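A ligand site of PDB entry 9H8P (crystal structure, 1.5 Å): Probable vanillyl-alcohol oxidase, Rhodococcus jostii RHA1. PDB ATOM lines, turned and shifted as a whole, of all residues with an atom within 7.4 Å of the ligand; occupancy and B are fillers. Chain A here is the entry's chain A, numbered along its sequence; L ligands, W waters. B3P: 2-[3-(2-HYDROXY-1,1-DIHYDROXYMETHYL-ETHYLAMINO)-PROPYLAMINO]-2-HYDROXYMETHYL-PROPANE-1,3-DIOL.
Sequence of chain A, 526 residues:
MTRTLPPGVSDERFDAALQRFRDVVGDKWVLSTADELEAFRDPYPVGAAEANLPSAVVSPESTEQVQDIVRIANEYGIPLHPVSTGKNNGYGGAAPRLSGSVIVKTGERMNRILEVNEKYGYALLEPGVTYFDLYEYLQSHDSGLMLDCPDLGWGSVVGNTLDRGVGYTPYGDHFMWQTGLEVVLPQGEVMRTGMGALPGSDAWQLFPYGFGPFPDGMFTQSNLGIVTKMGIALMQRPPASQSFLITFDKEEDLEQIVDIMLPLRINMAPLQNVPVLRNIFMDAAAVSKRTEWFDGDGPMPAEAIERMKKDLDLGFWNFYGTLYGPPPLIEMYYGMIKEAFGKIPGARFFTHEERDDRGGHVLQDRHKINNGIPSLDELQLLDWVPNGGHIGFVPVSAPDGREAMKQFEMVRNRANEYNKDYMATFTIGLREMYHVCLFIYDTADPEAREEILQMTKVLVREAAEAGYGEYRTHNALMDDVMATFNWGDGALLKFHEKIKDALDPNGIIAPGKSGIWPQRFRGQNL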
ATOM      1  N   ALA A  34     -33.363  13.799  -5.165  1.00  0.00           N
ATOM      2  CA  ALA A  34     -33.061  14.859  -6.105  1.00  0.00           C
ATOM      3  C   ALA A  34     -31.556  15.018  -6.288  1.00  0.00           C
ATOM      4  O   ALA A  34     -31.067  15.185  -7.391  1.00  0.00           O
ATOM      5  CB  ALA A  34     -33.680  16.154  -5.638  1.00  0.00           C
ATOM      6  N   LEU A  37     -29.956  12.281  -8.265  1.00  0.00           N
ATOM      7  CA  LEU A  37     -30.340  12.275  -9.673  1.00  0.00           C
ATOM      8  C   LEU A  37     -29.679  13.395 -10.460  1.00  0.00           C
ATOM      9  O   LEU A  37     -29.636  13.352 -11.679  1.00  0.00           O
ATOM     10  CB  LEU A  37     -31.848  12.304  -9.806  1.00  0.00           C
ATOM     11  CG  LEU A  37     -32.550  11.016  -9.290  1.00  0.00           C
ATOM     12  CD1 LEU A  37     -34.029  11.188  -9.314  1.00  0.00           C
ATOM     13  CD2 LEU A  37     -32.173   9.844 -10.111  1.00  0.00           C
ATOM     14  N   GLU A  38     -29.122  14.407  -9.807  1.00  0.00           N
ATOM     15  CA  GLU A  38     -28.509  15.555 -10.490  1.00  0.00           C
ATOM     16  C   GLU A  38     -27.431  15.101 -11.434  1.00  0.00           C
ATOM     17  O   GLU A  38     -27.386  15.664 -12.557  1.00  0.00           O
ATOM     18  CB  GLU A  38     -27.985  16.486  -9.378  1.00  0.00           C
ATOM     19  CG  GLU A  38     -27.008  17.572  -9.795  1.00  0.00           C
ATOM     20  CD  GLU A  38     -27.616  18.617 -10.670  1.00  0.00           C
ATOM     21  OE1 GLU A  38     -28.840  18.755 -10.698  1.00  0.00           O
ATOM     22  OE2 GLU A  38     -26.764  19.217 -11.422  1.00  0.00           O
ATOM     23  N   ALA A  39     -26.623  14.081 -11.067  1.00  0.00           N
ATOM     24  CA  ALA A  39     -25.541  13.651 -11.927  1.00  0.00           C
ATOM     25  C   ALA A  39     -25.995  12.938 -13.192  1.00  0.00           C
ATOM     26  O   ALA A  39     -25.200  12.632 -14.067  1.00  0.00           O
ATOM     27  CB  ALA A  39     -24.580  12.758 -11.168  1.00  0.00           C
ATOM     28  N   ARG A  41     -28.819  14.032 -14.894  1.00  0.00           N
ATOM     29  CA  ARG A  41     -29.387  15.007 -15.811  1.00  0.00           C
ATOM     30  C   ARG A  41     -28.380  15.230 -16.941  1.00  0.00           C
ATOM     31  O   ARG A  41     -27.175  14.994 -16.769  1.00  0.00           O
ATOM     32  CB  ARG A  41     -29.731  16.314 -15.125  1.00  0.00           C
ATOM     33  CG  ARG A  41     -30.892  16.148 -14.169  1.00  0.00           C
ATOM     34  CD  ARG A  41     -31.240  17.414 -13.428  1.00  0.00           C
ATOM     35  NE  ARG A  41     -32.460  17.186 -12.650  1.00  0.00           N
ATOM     36  CZ  ARG A  41     -33.289  18.157 -12.236  1.00  0.00           C
ATOM     37  NH1 ARG A  41     -33.052  19.437 -12.519  1.00  0.00           N
ATOM     38  NH2 ARG A  41     -34.419  17.832 -11.604  1.00  0.00           N
ATOM     39  N   ASP A  42     -28.882  15.689 -18.085  1.00  0.00           N
ATOM     40  CA  ASP A  42     -28.016  15.992 -19.202  1.00  0.00           C
ATOM     41  C   ASP A  42     -26.976  16.992 -18.731  1.00  0.00           C
ATOM     42  O   ASP A  42     -27.361  18.095 -18.294  1.00  0.00           O
ATOM     43  CB  ASP A  42     -28.863  16.526 -20.329  1.00  0.00           C
ATOM     44  CG  ASP A  42     -28.176  16.724 -21.672  1.00  0.00           C
ATOM     45  OD1 ASP A  42     -26.942  16.654 -21.709  1.00  0.00           O
ATOM     46  OD2 ASP A  42     -28.893  16.986 -22.652  1.00  0.00           O
ATOM     47  N   PRO A  43     -25.659  16.722 -18.874  1.00  0.00           N
ATOM     48  CA  PRO A  43     -24.670  17.716 -18.495  1.00  0.00           C
ATOM     49  C   PRO A  43     -24.668  18.947 -19.379  1.00  0.00           C
ATOM     50  O   PRO A  43     -24.196  20.014 -18.995  1.00  0.00           O
ATOM     51  CB  PRO A  43     -23.370  16.970 -18.556  1.00  0.00           C
ATOM     52  CG  PRO A  43     -23.590  15.909 -19.548  1.00  0.00           C
ATOM     53  CD  PRO A  43     -25.034  15.506 -19.379  1.00  0.00           C
ATOM     54  N   TYR A  44     -25.139  18.769 -20.624  1.00  0.00           N
ATOM     55  CA  TYR A  44     -25.127  19.801 -21.641  1.00  0.00           C
ATOM     56  C   TYR A  44     -26.571  20.041 -22.080  1.00  0.00           C
ATOM     57  O   TYR A  44     -27.001  19.681 -23.168  1.00  0.00           O
ATOM     58  CB  TYR A  44     -24.258  19.356 -22.833  1.00  0.00           C
ATOM     59  CG  TYR A  44     -22.812  18.961 -22.540  1.00  0.00           C
ATOM     60  CD1 TYR A  44     -22.130  19.333 -21.390  1.00  0.00           C
ATOM     61  CD2 TYR A  44     -22.156  18.109 -23.441  1.00  0.00           C
ATOM     62  CE1 TYR A  44     -20.816  18.940 -21.182  1.00  0.00           C
ATOM     63  CE2 TYR A  44     -20.852  17.726 -23.224  1.00  0.00           C
ATOM     64  CZ  TYR A  44     -20.180  18.117 -22.084  1.00  0.00           C
ATOM     65  OH  TYR A  44     -18.890  17.765 -21.788  1.00  0.00           O
ATOM     66  N   PRO A  45     -27.386  20.611 -21.185  1.00  0.00           N
ATOM     67  CA  PRO A  45     -28.819  20.717 -21.451  1.00  0.00           C
ATOM     68  C   PRO A  45     -29.120  21.632 -22.631  1.00  0.00           C
ATOM     69  O   PRO A  45     -28.414  22.653 -22.813  1.00  0.00           O
ATOM     70  CB  PRO A  45     -29.379  21.284 -20.171  1.00  0.00           C
ATOM     71  CG  PRO A  45     -28.223  22.003 -19.528  1.00  0.00           C
ATOM     72  CD  PRO A  45     -27.005  21.134 -19.878  1.00  0.00           C
ATOM     73  N   GLY A  47     -32.314  23.813 -24.403  1.00  0.00           N
ATOM     74  CA  GLY A  47     -33.573  24.463 -24.041  1.00  0.00           C
ATOM     75  C   GLY A  47     -33.494  25.057 -22.646  1.00  0.00           C
ATOM     76  O   GLY A  47     -32.836  24.501 -21.767  1.00  0.00           O
ATOM     77  N   ALA A  48     -34.168  26.214 -22.435  1.00  0.00           N
ATOM     78  CA  ALA A  48     -34.158  26.851 -21.146  1.00  0.00           C
ATOM     79  C   ALA A  48     -34.966  26.029 -20.142  1.00  0.00           C
ATOM     80  O   ALA A  48     -34.534  25.898 -18.979  1.00  0.00           O
ATOM     81  CB  ALA A  48     -34.716  28.243 -21.225  1.00  0.00           C
ATOM     82  N   ALA A  49     -36.123  25.521 -20.568  1.00  0.00           N
ATOM     83  CA  ALA A  49     -36.971  24.748 -19.676  1.00  0.00           C
ATOM     84  C   ALA A  49     -36.322  23.404 -19.368  1.00  0.00           C
ATOM     85  O   ALA A  49     -35.635  22.811 -20.200  1.00  0.00           O
ATOM     86  CB  ALA A  49     -38.348  24.553 -20.237  1.00  0.00           C
ATOM     87  N   GLU A  50     -36.532  22.908 -18.154  1.00  0.00           N
ATOM     88  CA  GLU A  50     -36.059  21.600 -17.798  1.00  0.00           C
ATOM     89  C   GLU A  50     -36.761  20.570 -18.685  1.00  0.00           C
ATOM     90  O   GLU A  50     -37.924  20.723 -19.048  1.00  0.00           O
ATOM     91  CB  GLU A  50     -36.294  21.298 -16.326  1.00  0.00           C
ATOM     92  CG  GLU A  50     -35.272  22.000 -15.437  1.00  0.00           C
ATOM     93  CD  GLU A  50     -33.811  21.638 -15.741  1.00  0.00           C
ATOM     94  OE1 GLU A  50     -33.466  20.906 -16.722  1.00  0.00           O
ATOM     95  OE2 GLU A  50     -32.994  22.084 -14.923  1.00  0.00           O
ATOM     96  N   ALA A  51     -36.010  19.538 -19.034  1.00  0.00           N
ATOM     97  CA  ALA A  51     -36.505  18.468 -19.868  1.00  0.00           C
ATOM     98  C   ALA A  51     -35.679  17.225 -19.555  1.00  0.00           C
ATOM     99  O   ALA A  51     -34.602  17.314 -18.926  1.00  0.00           O
ATOM    100  CB  ALA A  51     -36.349  18.813 -21.356  1.00  0.00           C
ATOM    101  N   LEU A  53     -35.945  14.549 -17.546  1.00  0.00           N
ATOM    102  CA  LEU A  53     -35.620  14.361 -16.139  1.00  0.00           C
ATOM    103  C   LEU A  53     -35.832  12.905 -15.742  1.00  0.00           C
ATOM    104  O   LEU A  53     -36.918  12.383 -15.904  1.00  0.00           O
ATOM    105  CB  LEU A  53     -36.517  15.243 -15.276  1.00  0.00           C
ATOM    106  CG  LEU A  53     -36.323  16.758 -15.515  1.00  0.00           C
ATOM    107  CD1 LEU A  53     -37.121  17.611 -14.607  1.00  0.00           C
ATOM    108  CD2 LEU A  53     -34.858  17.180 -15.495  1.00  0.00           C
ATOM    109  N   LEU A 382     -14.487  21.973 -24.020  1.00  0.00           N
ATOM    110  CA  LEU A 382     -15.545  22.549 -23.223  1.00  0.00           C
ATOM    111  C   LEU A 382     -15.091  23.780 -22.445  1.00  0.00           C
ATOM    112  O   LEU A 382     -15.928  24.446 -21.839  1.00  0.00           O
ATOM    113  CB  LEU A 382     -16.191  21.508 -22.311  1.00  0.00           C
ATOM    114  CG  LEU A 382     -17.072  20.461 -22.989  1.00  0.00           C
ATOM    115  CD1 LEU A 382     -17.985  21.070 -24.027  1.00  0.00           C
ATOM    116  CD2 LEU A 382     -16.344  19.303 -23.632  1.00  0.00           C
ATOM    117  N   PRO A 386     -17.367  29.689 -20.577  1.00  0.00           N
ATOM    118  CA  PRO A 386     -17.671  29.249 -19.223  1.00  0.00           C
ATOM    119  C   PRO A 386     -18.772  28.201 -19.152  1.00  0.00           C
ATOM    120  O   PRO A 386     -19.695  28.238 -19.936  1.00  0.00           O
ATOM    121  CB  PRO A 386     -18.123  30.527 -18.536  1.00  0.00           C
ATOM    122  CG  PRO A 386     -17.457  31.623 -19.366  1.00  0.00           C
ATOM    123  CD  PRO A 386     -17.492  31.138 -20.767  1.00  0.00           C
ATOM    124  N   ASN A 387     -18.626  27.264 -18.215  1.00  0.00           N
ATOM    125  CA  ASN A 387     -19.635  26.234 -17.988  1.00  0.00           C
ATOM    126  C   ASN A 387     -19.957  25.485 -19.278  1.00  0.00           C
ATOM    127  O   ASN A 387     -21.122  25.172 -19.584  1.00  0.00           O
ATOM    128  CB  ASN A 387     -20.914  26.846 -17.398  1.00  0.00           C
ATOM    129  CG  ASN A 387     -20.636  27.808 -16.279  1.00  0.00           C
ATOM    130  OD1 ASN A 387     -20.064  27.409 -15.277  1.00  0.00           O
ATOM    131  ND2 ASN A 387     -20.985  29.068 -16.462  1.00  0.00           N
ATOM    132  N   GLY A 388     -18.909  25.246 -20.081  1.00  0.00           N
ATOM    133  CA  GLY A 388     -19.096  24.785 -21.449  1.00  0.00           C
ATOM    134  C   GLY A 388     -19.767  23.439 -21.569  1.00  0.00           C
ATOM    135  O   GLY A 388     -19.507  22.494 -20.825  1.00  0.00           O
ATOM    136  N   GLY A 389     -20.653  23.376 -22.554  1.00  0.00           N
ATOM    137  CA  GLY A 389     -21.246  22.143 -23.023  1.00  0.00           C
ATOM    138  C   GLY A 389     -21.340  22.195 -24.536  1.00  0.00           C
ATOM    139  O   GLY A 389     -21.076  23.243 -25.138  1.00  0.00           O
ATOM    140  N   ASP A 442     -22.529  28.138 -23.026  1.00  0.00           N
ATOM    141  CA  ASP A 442     -22.604  28.246 -21.569  1.00  0.00           C
ATOM    142  C   ASP A 442     -23.857  27.574 -21.035  1.00  0.00           C
ATOM    143  O   ASP A 442     -24.949  28.110 -21.147  1.00  0.00           O
ATOM    144  CB  ASP A 442     -22.487  29.711 -21.191  1.00  0.00           C
ATOM    145  CG  ASP A 442     -22.498  29.981 -19.696  1.00  0.00           C
ATOM    146  OD1 ASP A 442     -22.815  29.090 -18.904  1.00  0.00           O
ATOM    147  OD2 ASP A 442     -22.125  31.134 -19.310  1.00  0.00           O
ATOM    148  N   THR A 443     -23.663  26.388 -20.460  1.00  0.00           N
ATOM    149  CA  THR A 443     -24.799  25.578 -20.012  1.00  0.00           C
ATOM    150  C   THR A 443     -25.509  26.185 -18.812  1.00  0.00           C
ATOM    151  O   THR A 443     -26.601  25.728 -18.491  1.00  0.00           O
ATOM    152  CB  THR A 443     -24.363  24.148 -19.652  1.00  0.00           C
ATOM    153  OG1 THR A 443     -23.478  24.207 -18.511  1.00  0.00           O
ATOM    154  CG2 THR A 443     -23.752  23.427 -20.831  1.00  0.00           C
ATOM    155  N   ALA A 444     -24.905  27.180 -18.152  1.00  0.00           N
ATOM    156  CA  ALA A 444     -25.543  27.821 -17.007  1.00  0.00           C
ATOM    157  C   ALA A 444     -26.460  28.959 -17.402  1.00  0.00           C
ATOM    158  O   ALA A 444     -27.136  29.532 -16.561  1.00  0.00           O
ATOM    159  CB  ALA A 444     -24.512  28.326 -16.022  1.00  0.00           C
ATOM    160  N   ARG A 449     -28.953  28.201 -23.581  1.00  0.00           N
ATOM    161  CA  ARG A 449     -29.597  26.894 -23.720  1.00  0.00           C
ATOM    162  C   ARG A 449     -30.745  26.996 -24.763  1.00  0.00           C
ATOM    163  O   ARG A 449     -30.938  26.085 -25.571  1.00  0.00           O
ATOM    164  CB  ARG A 449     -30.173  26.402 -22.370  1.00  0.00           C
ATOM    165  CG  ARG A 449     -29.068  25.975 -21.419  1.00  0.00           C
ATOM    166  CD  ARG A 449     -29.644  25.537 -20.059  1.00  0.00           C
ATOM    167  NE  ARG A 449     -30.858  24.752 -19.936  1.00  0.00           N
ATOM    168  CZ  ARG A 449     -31.161  23.977 -18.872  1.00  0.00           C
ATOM    169  NH1 ARG A 449     -30.439  24.030 -17.741  1.00  0.00           N
ATOM    170  NH2 ARG A 449     -32.188  23.130 -18.923  1.00  0.00           N
HETATM  171  C1  B3P L   1     -25.984  22.154 -16.631  1.00  0.00           C
HETATM  172  C2  B3P L   1     -27.091  22.509 -15.706  1.00  0.00           C
HETATM  173  C3  B3P L   1     -24.687  21.767 -15.957  1.00  0.00           C
HETATM  174  N1  B3P L   1     -23.532  21.698 -16.888  1.00  0.00           N
HETATM  175  C4  B3P L   1     -22.205  21.390 -16.287  1.00  0.00           C
HETATM  176  C5  B3P L   1     -21.731  22.496 -15.317  1.00  0.00           C
HETATM  177  C6  B3P L   1     -21.176  21.187 -17.403  1.00  0.00           C
HETATM  178  C7  B3P L   1     -22.235  20.124 -15.433  1.00  0.00           C
HETATM  179  N2  B3P L   1     -27.815  21.330 -15.208  1.00  0.00           N
HETATM  180  C8  B3P L   1     -28.673  21.582 -14.013  1.00  0.00           C
HETATM  181  C9  B3P L   1     -29.232  20.218 -13.605  1.00  0.00           C
HETATM  182  C10 B3P L   1     -29.785  22.566 -14.371  1.00  0.00           C
HETATM  183  C11 B3P L   1     -27.813  22.167 -12.873  1.00  0.00           C
HETATM  184  O1  B3P L   1     -30.108  20.305 -12.486  1.00  0.00           O
HETATM  185  O2  B3P L   1     -30.520  22.171 -15.536  1.00  0.00           O
HETATM  186  O3  B3P L   1     -26.587  21.481 -12.686  1.00  0.00           O
HETATM  187  O4  B3P L   1     -21.843  23.764 -15.910  1.00  0.00           O
HETATM  188  O5  B3P L   1     -19.889  20.853 -16.883  1.00  0.00           O
HETATM  189  O6  B3P L   1     -22.873  19.052 -16.106  1.00  0.00           O
HETATM  190  O   HOH W   1     -23.180  16.798 -14.730  1.00  0.00           O
HETATM  191  O   HOH W   2     -29.064  19.659 -17.080  1.00  0.00           O
HETATM  192  O   HOH W   3     -26.405  18.951 -15.439  1.00  0.00           O
HETATM  193  O   HOH W   4     -18.051  21.613 -18.789  1.00  0.00           O
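An oxygen (O2) of the ligand lies within hydrogen-bond range of the side-chain carboxylate (OE2) of Glu 50, 2.6 Å away. The side-chain carboxylate (OE2) of Glu 38 lies within hydrogen-bond range of an oxygen (O3) of the ligand, at 2.6 Å. A nitrogen (N1) of the ligand is in hydrogen-bond range of the backbone carbonyl oxygen of Pro 43, 2.8 Å away. An oxygen (O2) of the ligand sits at hydrogen-bond distance from the guanidinium group (NH1) of Arg 449, at 2.9 Å. The side-chain hydroxyl (OG1) of Thr 443 sits at hydrogen-bond distance from a nitrogen (N1) of the ligand (3.0 Å). The guanidinium group of Arg 41 is in hydrogen-bond range of an oxygen (O1) of the ligand, 3.1 Å away.
OE1 of Glu 50 lies within salt-bridge range of NH2 of Arg 449. The side-chain carboxylate (OE2) of Glu 50 lies within salt-bridge range of the guanidinium group (NH1) of Arg 41, 3.6 Å away. The guanidinium group (NE) of Arg 449 is in hydrogen-bond range of the backbone carbonyl oxygen (O) of Gly 47, at 2.7 Å. OG1 of Thr 443 sits at hydrogen-bond distance from O of Asn 387. ND2 of Asn 387 sits at hydrogen-bond distance from OD1 of Asp 442, at 3.1 Å.
CD of Pro 45 touches C1 of the ligand, 3.6 Å away. Asn 387 touches the ligand. Hydrophobic or aromatic side chains that line the ligand: Pro 43 and Pro 45.
Water W4 bridges the backbone carbonyl oxygen (O) of Gly 388 (2.7 Å) and an oxygen (O5) of the ligand (2.8 Å). Water W3 lies within hydrogen-bond range of a nitrogen (N2) of the ligand (2.8 Å) and the backbone carbonyl oxygen of Asp 42 (3.1 Å). Water W2 bridges the backbone carbonyl oxygen (O) of Asp 42 (2.6 Å) and a nitrogen (N2) of the ligand (2.8 Å).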
